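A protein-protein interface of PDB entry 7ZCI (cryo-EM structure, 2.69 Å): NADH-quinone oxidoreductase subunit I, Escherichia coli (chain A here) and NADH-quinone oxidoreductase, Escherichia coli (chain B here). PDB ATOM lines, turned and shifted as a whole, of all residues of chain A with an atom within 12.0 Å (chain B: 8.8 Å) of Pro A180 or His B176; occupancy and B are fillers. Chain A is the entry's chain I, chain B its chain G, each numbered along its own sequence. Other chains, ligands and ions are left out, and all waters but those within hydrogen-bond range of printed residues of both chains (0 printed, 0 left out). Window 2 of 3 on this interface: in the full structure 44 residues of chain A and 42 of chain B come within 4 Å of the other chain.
O of Ile A173 lies within hydrogen-bond range of ND2 of Asn B178 (2.8 Å).
The backbone NH of Tyr B173 is in hydrogen-bond range of the backbone carbonyl oxygen of Tyr B180 (2.8 Å). The side-chain carboxylate (OD1) of Asp B177 lies within hydrogen-bond range of a ring nitrogen (ND1) of His B176, 2.8 Å away. The backbone NH (N) of Lys A176 lies close to the side-chain carboxylate (OD1) of Asp A174, at 3.2 Å. The side-chain hydroxyl (OG) of Ser A177 lies within hydrogen-bond range of the backbone carbonyl oxygen (O) of Asp A174.
Among the printed residues, pairs that only touch across the chains: Val A175 with Asn B178, Pro A180 with His B176, Val A175 with Gly B174, Val A175 with Tyr B180, Asp A174 with Asn B178 and Val A175 with Tyr B173.
Pro A180 touches one residue of chain B. Of chain A, only Pro A180 comes within 4 Å of His B176. Gly B174 touches just one residue of chain A: Val A175 (3.5 Å). No residue of chain A comes within 4 Å of Ala B175. Of chain A, only Ile A173 (2.8 Å), Asp A174 (3.9 Å) and Val A175 (3.5 Å) come within 4 Å of Asn B178. No residue of chain A comes within 4 Å of Val B179. Printed residues of chain A within 4 Å of Tyr B180: Val A175. Printed residues of chain B within 4 Å of Ile A173: Asn B178 (2.8 Å). Printed residues of chain B within 4 Å of Val A175: Tyr B173, Gly B174, Asn B178 and Tyr B180. The nearest residue of chain B that does not touch Pro A180 is Ala B175 (6.4 Å). The nearest printed residue of chain A that does not touch Tyr B173 is Lys A176 (7.2 Å).
Of the 12 printed residues of chain B, 5 touch a printed residue of chain A. Hydrophobic or aromatic side chains of chain B that line the printed part of chain A: Tyr B173, His B176 and Tyr B180. Printed residues of chain A that touch a printed residue of chain B: Ile A173, Asp A174, Val A175 and Pro A180. Hydrophobic or aromatic side chains of chain A that line the printed part of chain B: Ile A173 and Val A175.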
ATOM      1  N   ALA A 170      28.932   3.453  -9.863  1.00  0.00           N
ATOM      2  CA  ALA A 170      29.120   2.319  -8.979  1.00  0.00           C
ATOM      3  C   ALA A 170      28.341   1.117  -9.498  1.00  0.00           C
ATOM      4  O   ALA A 170      27.378   1.246 -10.257  1.00  0.00           O
ATOM      5  CB  ALA A 170      28.681   2.657  -7.559  1.00  0.00           C
ATOM      6  N   LYS A 171      28.781  -0.065  -9.085  1.00  0.00           N
ATOM      7  CA  LYS A 171      28.096  -1.289  -9.454  1.00  0.00           C
ATOM      8  C   LYS A 171      26.727  -1.342  -8.779  1.00  0.00           C
ATOM      9  O   LYS A 171      26.552  -0.814  -7.680  1.00  0.00           O
ATOM     10  CB  LYS A 171      28.928  -2.508  -9.058  1.00  0.00           C
ATOM     11  CG  LYS A 171      29.744  -3.173 -10.176  1.00  0.00           C
ATOM     12  CD  LYS A 171      30.403  -2.223 -11.187  1.00  0.00           C
ATOM     13  CE  LYS A 171      31.479  -1.318 -10.569  1.00  0.00           C
ATOM     14  NZ  LYS A 171      31.882  -0.209 -11.478  1.00  0.00           N
ATOM     15  N   PRO A 172      25.733  -1.947  -9.431  1.00  0.00           N
ATOM     16  CA  PRO A 172      24.384  -1.990  -8.849  1.00  0.00           C
ATOM     17  C   PRO A 172      24.335  -2.881  -7.617  1.00  0.00           C
ATOM     18  O   PRO A 172      24.592  -4.083  -7.688  1.00  0.00           O
ATOM     19  CB  PRO A 172      23.522  -2.544  -9.988  1.00  0.00           C
ATOM     20  CG  PRO A 172      24.465  -3.229 -10.887  1.00  0.00           C
ATOM     21  CD  PRO A 172      25.755  -2.493 -10.798  1.00  0.00           C
ATOM     22  N   ILE A 173      24.024  -2.273  -6.478  1.00  0.00           N
ATOM     23  CA  ILE A 173      23.829  -3.019  -5.240  1.00  0.00           C
ATOM     24  C   ILE A 173      22.432  -3.613  -5.266  1.00  0.00           C
ATOM     25  O   ILE A 173      21.442  -2.881  -5.348  1.00  0.00           O
ATOM     26  CB  ILE A 173      24.014  -2.119  -4.013  1.00  0.00           C
ATOM     27  CG1 ILE A 173      25.415  -1.522  -3.989  1.00  0.00           C
ATOM     28  CG2 ILE A 173      23.729  -2.894  -2.748  1.00  0.00           C
ATOM     29  CD1 ILE A 173      25.563  -0.405  -3.004  1.00  0.00           C
ATOM     30  N   ASP A 174      22.347  -4.938  -5.201  1.00  0.00           N
ATOM     31  CA  ASP A 174      21.047  -5.583  -5.160  1.00  0.00           C
ATOM     32  C   ASP A 174      20.348  -5.263  -3.849  1.00  0.00           C
ATOM     33  O   ASP A 174      20.972  -5.161  -2.793  1.00  0.00           O
ATOM     34  CB  ASP A 174      21.173  -7.094  -5.325  1.00  0.00           C
ATOM     35  CG  ASP A 174      19.901  -7.722  -5.854  1.00  0.00           C
ATOM     36  OD1 ASP A 174      18.928  -7.831  -5.085  1.00  0.00           O
ATOM     37  OD2 ASP A 174      19.869  -8.100  -7.042  1.00  0.00           O
ATOM     38  N   VAL A 175      19.030  -5.098  -3.936  1.00  0.00           N
ATOM     39  CA  VAL A 175      18.249  -4.640  -2.799  1.00  0.00           C
ATOM     40  C   VAL A 175      18.182  -5.697  -1.702  1.00  0.00           C
ATOM     41  O   VAL A 175      17.918  -5.368  -0.542  1.00  0.00           O
ATOM     42  CB  VAL A 175      16.864  -4.206  -3.324  1.00  0.00           C
ATOM     43  CG1 VAL A 175      15.763  -5.191  -2.962  1.00  0.00           C
ATOM     44  CG2 VAL A 175      16.554  -2.813  -2.896  1.00  0.00           C
ATOM     45  N   LYS A 176      18.470  -6.953  -2.039  1.00  0.00           N
ATOM     46  CA  LYS A 176      18.486  -8.065  -1.107  1.00  0.00           C
ATOM     47  C   LYS A 176      19.865  -8.321  -0.516  1.00  0.00           C
ATOM     48  O   LYS A 176      20.108  -9.412   0.003  1.00  0.00           O
ATOM     49  CB  LYS A 176      17.979  -9.328  -1.801  1.00  0.00           C
ATOM     50  CG  LYS A 176      16.617  -9.162  -2.435  1.00  0.00           C
ATOM     51  CD  LYS A 176      16.059 -10.479  -2.923  1.00  0.00           C
ATOM     52  CE  LYS A 176      17.029 -11.211  -3.822  1.00  0.00           C
ATOM     53  NZ  LYS A 176      16.396 -11.567  -5.117  1.00  0.00           N
ATOM     54  N   SER A 177      20.771  -7.352  -0.593  1.00  0.00           N
ATOM     55  CA  SER A 177      22.123  -7.550  -0.093  1.00  0.00           C
ATOM     56  C   SER A 177      22.142  -7.581   1.430  1.00  0.00           C
ATOM     57  O   SER A 177      21.339  -6.927   2.097  1.00  0.00           O
ATOM     58  CB  SER A 177      23.048  -6.447  -0.596  1.00  0.00           C
ATOM     59  OG  SER A 177      22.646  -5.190  -0.093  1.00  0.00           O
ATOM     60  N   LEU A 178      23.084  -8.354   1.974  1.00  0.00           N
ATOM     61  CA  LEU A 178      23.175  -8.525   3.418  1.00  0.00           C
ATOM     62  C   LEU A 178      23.703  -7.281   4.112  1.00  0.00           C
ATOM     63  O   LEU A 178      23.427  -7.075   5.298  1.00  0.00           O
ATOM     64  CB  LEU A 178      24.071  -9.716   3.748  1.00  0.00           C
ATOM     65  CG  LEU A 178      23.692 -11.040   3.099  1.00  0.00           C
ATOM     66  CD1 LEU A 178      24.779 -12.069   3.322  1.00  0.00           C
ATOM     67  CD2 LEU A 178      22.373 -11.515   3.659  1.00  0.00           C
ATOM     68  N   LEU A 179      24.467  -6.461   3.406  1.00  0.00           N
ATOM     69  CA  LEU A 179      25.096  -5.307   4.024  1.00  0.00           C
ATOM     70  C   LEU A 179      24.051  -4.243   4.355  1.00  0.00           C
ATOM     71  O   LEU A 179      23.099  -4.053   3.595  1.00  0.00           O
ATOM     72  CB  LEU A 179      26.161  -4.731   3.097  1.00  0.00           C
ATOM     73  CG  LEU A 179      27.437  -5.566   3.000  1.00  0.00           C
ATOM     74  CD1 LEU A 179      28.312  -5.080   1.869  1.00  0.00           C
ATOM     75  CD2 LEU A 179      28.187  -5.512   4.309  1.00  0.00           C
ATOM     76  N   PRO A 180      24.197  -3.538   5.486  1.00  0.00           N
ATOM     77  CA  PRO A 180      23.260  -2.484   5.889  1.00  0.00           C
ATOM     78  C   PRO A 180      23.261  -1.279   4.949  1.00  0.00           C
ATOM     79  O   PRO A 180      24.285  -0.993   4.324  1.00  0.00           O
ATOM     80  CB  PRO A 180      23.767  -2.078   7.275  1.00  0.00           C
ATOM     81  CG  PRO A 180      24.591  -3.207   7.730  1.00  0.00           C
ATOM     82  CD  PRO A 180      25.221  -3.773   6.514  1.00  0.00           C
ATOM     83  N   ASN B  98      23.098  11.294  -8.407  1.00  0.00           N
ATOM     84  CA  ASN B  98      23.041   9.914  -8.865  1.00  0.00           C
ATOM     85  C   ASN B  98      22.368   9.743 -10.217  1.00  0.00           C
ATOM     86  O   ASN B  98      22.344   8.626 -10.733  1.00  0.00           O
ATOM     87  CB  ASN B  98      22.307   9.044  -7.841  1.00  0.00           C
ATOM     88  CG  ASN B  98      23.095   8.841  -6.583  1.00  0.00           C
ATOM     89  OD1 ASN B  98      24.100   8.138  -6.575  1.00  0.00           O
ATOM     90  ND2 ASN B  98      22.647   9.455  -5.504  1.00  0.00           N
ATOM     91  N   ARG B 133      25.087   5.765  -7.998  1.00  0.00           N
ATOM     92  CA  ARG B 133      24.496   4.457  -7.781  1.00  0.00           C
ATOM     93  C   ARG B 133      23.758   4.002  -9.034  1.00  0.00           C
ATOM     94  O   ARG B 133      23.264   4.810  -9.821  1.00  0.00           O
ATOM     95  CB  ARG B 133      23.547   4.485  -6.584  1.00  0.00           C
ATOM     96  CG  ARG B 133      22.311   5.347  -6.756  1.00  0.00           C
ATOM     97  CD  ARG B 133      21.065   4.516  -7.010  1.00  0.00           C
ATOM     98  NE  ARG B 133      19.933   5.334  -7.422  1.00  0.00           N
ATOM     99  CZ  ARG B 133      19.723   5.771  -8.655  1.00  0.00           C
ATOM    100  NH1 ARG B 133      20.562   5.502  -9.639  1.00  0.00           N
ATOM    101  NH2 ARG B 133      18.634   6.485  -8.911  1.00  0.00           N
ATOM    102  N   ALA B 153      13.166   8.777  -6.343  1.00  0.00           N
ATOM    103  CA  ALA B 153      12.523   8.323  -5.110  1.00  0.00           C
ATOM    104  C   ALA B 153      11.508   9.348  -4.611  1.00  0.00           C
ATOM    105  O   ALA B 153      11.496   9.744  -3.447  1.00  0.00           O
ATOM    106  CB  ALA B 153      13.552   7.976  -4.036  1.00  0.00           C
ATOM    107  N   TYR B 155       8.281   8.724  -4.772  1.00  0.00           N
ATOM    108  CA  TYR B 155       7.231   7.851  -4.248  1.00  0.00           C
ATOM    109  C   TYR B 155       5.880   8.046  -4.915  1.00  0.00           C
ATOM    110  O   TYR B 155       4.889   7.515  -4.421  1.00  0.00           O
ATOM    111  CB  TYR B 155       7.064   7.990  -2.730  1.00  0.00           C
ATOM    112  CG  TYR B 155       8.253   7.515  -1.946  1.00  0.00           C
ATOM    113  CD1 TYR B 155       9.307   8.369  -1.670  1.00  0.00           C
ATOM    114  CD2 TYR B 155       8.333   6.210  -1.491  1.00  0.00           C
ATOM    115  CE1 TYR B 155      10.404   7.939  -0.964  1.00  0.00           C
ATOM    116  CE2 TYR B 155       9.423   5.773  -0.782  1.00  0.00           C
ATOM    117  CZ  TYR B 155      10.459   6.640  -0.523  1.00  0.00           C
ATOM    118  OH  TYR B 155      11.553   6.218   0.184  1.00  0.00           O
ATOM    119  N   TYR B 173      11.171  -1.157  -2.178  1.00  0.00           N
ATOM    120  CA  TYR B 173      12.024  -2.113  -1.498  1.00  0.00           C
ATOM    121  C   TYR B 173      13.324  -1.440  -1.107  1.00  0.00           C
ATOM    122  O   TYR B 173      13.658  -0.359  -1.588  1.00  0.00           O
ATOM    123  CB  TYR B 173      12.308  -3.328  -2.375  1.00  0.00           C
ATOM    124  CG  TYR B 173      11.104  -3.741  -3.152  1.00  0.00           C
ATOM    125  CD1 TYR B 173      10.056  -4.385  -2.524  1.00  0.00           C
ATOM    126  CD2 TYR B 173      10.998  -3.468  -4.503  1.00  0.00           C
ATOM    127  CE1 TYR B 173       8.943  -4.754  -3.213  1.00  0.00           C
ATOM    128  CE2 TYR B 173       9.887  -3.833  -5.201  1.00  0.00           C
ATOM    129  CZ  TYR B 173       8.860  -4.473  -4.548  1.00  0.00           C
ATOM    130  OH  TYR B 173       7.738  -4.840  -5.232  1.00  0.00           O
ATOM    131  N   GLY B 174      14.039  -2.084  -0.208  1.00  0.00           N
ATOM    132  CA  GLY B 174      15.325  -1.581   0.191  1.00  0.00           C
ATOM    133  C   GLY B 174      15.229  -0.386   1.109  1.00  0.00           C
ATOM    134  O   GLY B 174      14.223  -0.132   1.766  1.00  0.00           O
ATOM    135  N   ALA B 175      16.309   0.376   1.117  1.00  0.00           N
ATOM    136  CA  ALA B 175      16.606   1.283   2.213  1.00  0.00           C
ATOM    137  C   ALA B 175      17.377   2.497   1.726  1.00  0.00           C
ATOM    138  O   ALA B 175      17.338   2.839   0.545  1.00  0.00           O
ATOM    139  CB  ALA B 175      17.374   0.558   3.317  1.00  0.00           C
ATOM    140  N   HIS B 176      18.152   3.072   2.635  1.00  0.00           N
ATOM    141  CA  HIS B 176      18.669   4.431   2.717  1.00  0.00           C
ATOM    142  C   HIS B 176      18.839   5.216   1.424  1.00  0.00           C
ATOM    143  O   HIS B 176      18.224   6.267   1.272  1.00  0.00           O
ATOM    144  CB  HIS B 176      20.031   4.299   3.387  1.00  0.00           C
ATOM    145  CG  HIS B 176      20.721   3.013   3.039  1.00  0.00           C
ATOM    146  ND1 HIS B 176      21.457   2.853   1.888  1.00  0.00           N
ATOM    147  CD2 HIS B 176      20.729   1.808   3.657  1.00  0.00           C
ATOM    148  CE1 HIS B 176      21.915   1.617   1.824  1.00  0.00           C
ATOM    149  NE2 HIS B 176      21.484   0.960   2.883  1.00  0.00           N
ATOM    150  N   ASP B 177      19.632   4.728   0.484  1.00  0.00           N
ATOM    151  CA  ASP B 177      19.741   5.386  -0.811  1.00  0.00           C
ATOM    152  C   ASP B 177      19.700   4.358  -1.922  1.00  0.00           C
ATOM    153  O   ASP B 177      19.870   4.717  -3.090  1.00  0.00           O
ATOM    154  CB  ASP B 177      21.011   6.241  -0.912  1.00  0.00           C
ATOM    155  CG  ASP B 177      22.285   5.411  -0.938  1.00  0.00           C
ATOM    156  OD1 ASP B 177      22.386   4.439  -0.163  1.00  0.00           O
ATOM    157  OD2 ASP B 177      23.198   5.749  -1.717  1.00  0.00           O
ATOM    158  N   ASN B 178      19.472   3.093  -1.583  1.00  0.00           N
ATOM    159  CA  ASN B 178      19.230   2.031  -2.543  1.00  0.00           C
ATOM    160  C   ASN B 178      17.750   1.690  -2.649  1.00  0.00           C
ATOM    161  O   ASN B 178      17.400   0.533  -2.888  1.00  0.00           O
ATOM    162  CB  ASN B 178      20.042   0.797  -2.155  1.00  0.00           C
ATOM    163  CG  ASN B 178      20.514   0.021  -3.344  1.00  0.00           C
ATOM    164  OD1 ASN B 178      20.976   0.591  -4.328  1.00  0.00           O
ATOM    165  ND2 ASN B 178      20.411  -1.295  -3.265  1.00  0.00           N
ATOM    166  N   VAL B 179      16.874   2.675  -2.444  1.00  0.00           N
ATOM    167  CA  VAL B 179      15.436   2.431  -2.480  1.00  0.00           C
ATOM    168  C   VAL B 179      15.013   2.103  -3.902  1.00  0.00           C
ATOM    169  O   VAL B 179      15.307   2.844  -4.846  1.00  0.00           O
ATOM    170  CB  VAL B 179      14.657   3.638  -1.934  1.00  0.00           C
ATOM    171  CG1 VAL B 179      14.309   3.414  -0.486  1.00  0.00           C
ATOM    172  CG2 VAL B 179      15.433   4.925  -2.111  1.00  0.00           C
ATOM    173  N   TYR B 180      14.312   0.994  -4.055  1.00  0.00           N
ATOM    174  CA  TYR B 180      13.960   0.433  -5.345  1.00  0.00           C
ATOM    175  C   TYR B 180      12.452   0.487  -5.520  1.00  0.00           C
ATOM    176  O   TYR B 180      11.706   0.217  -4.584  1.00  0.00           O
ATOM    177  CB  TYR B 180      14.466  -0.999  -5.449  1.00  0.00           C
ATOM    178  CG  TYR B 180      14.525  -1.540  -6.843  1.00  0.00           C
ATOM    179  CD1 TYR B 180      13.415  -2.125  -7.427  1.00  0.00           C
ATOM    180  CD2 TYR B 180      15.694  -1.475  -7.576  1.00  0.00           C
ATOM    181  CE1 TYR B 180      13.469  -2.626  -8.700  1.00  0.00           C
ATOM    182  CE2 TYR B 180      15.757  -1.972  -8.848  1.00  0.00           C
ATOM    183  CZ  TYR B 180      14.642  -2.549  -9.405  1.00  0.00           C
ATOM    184  OH  TYR B 180      14.695  -3.045 -10.678  1.00  0.00           O
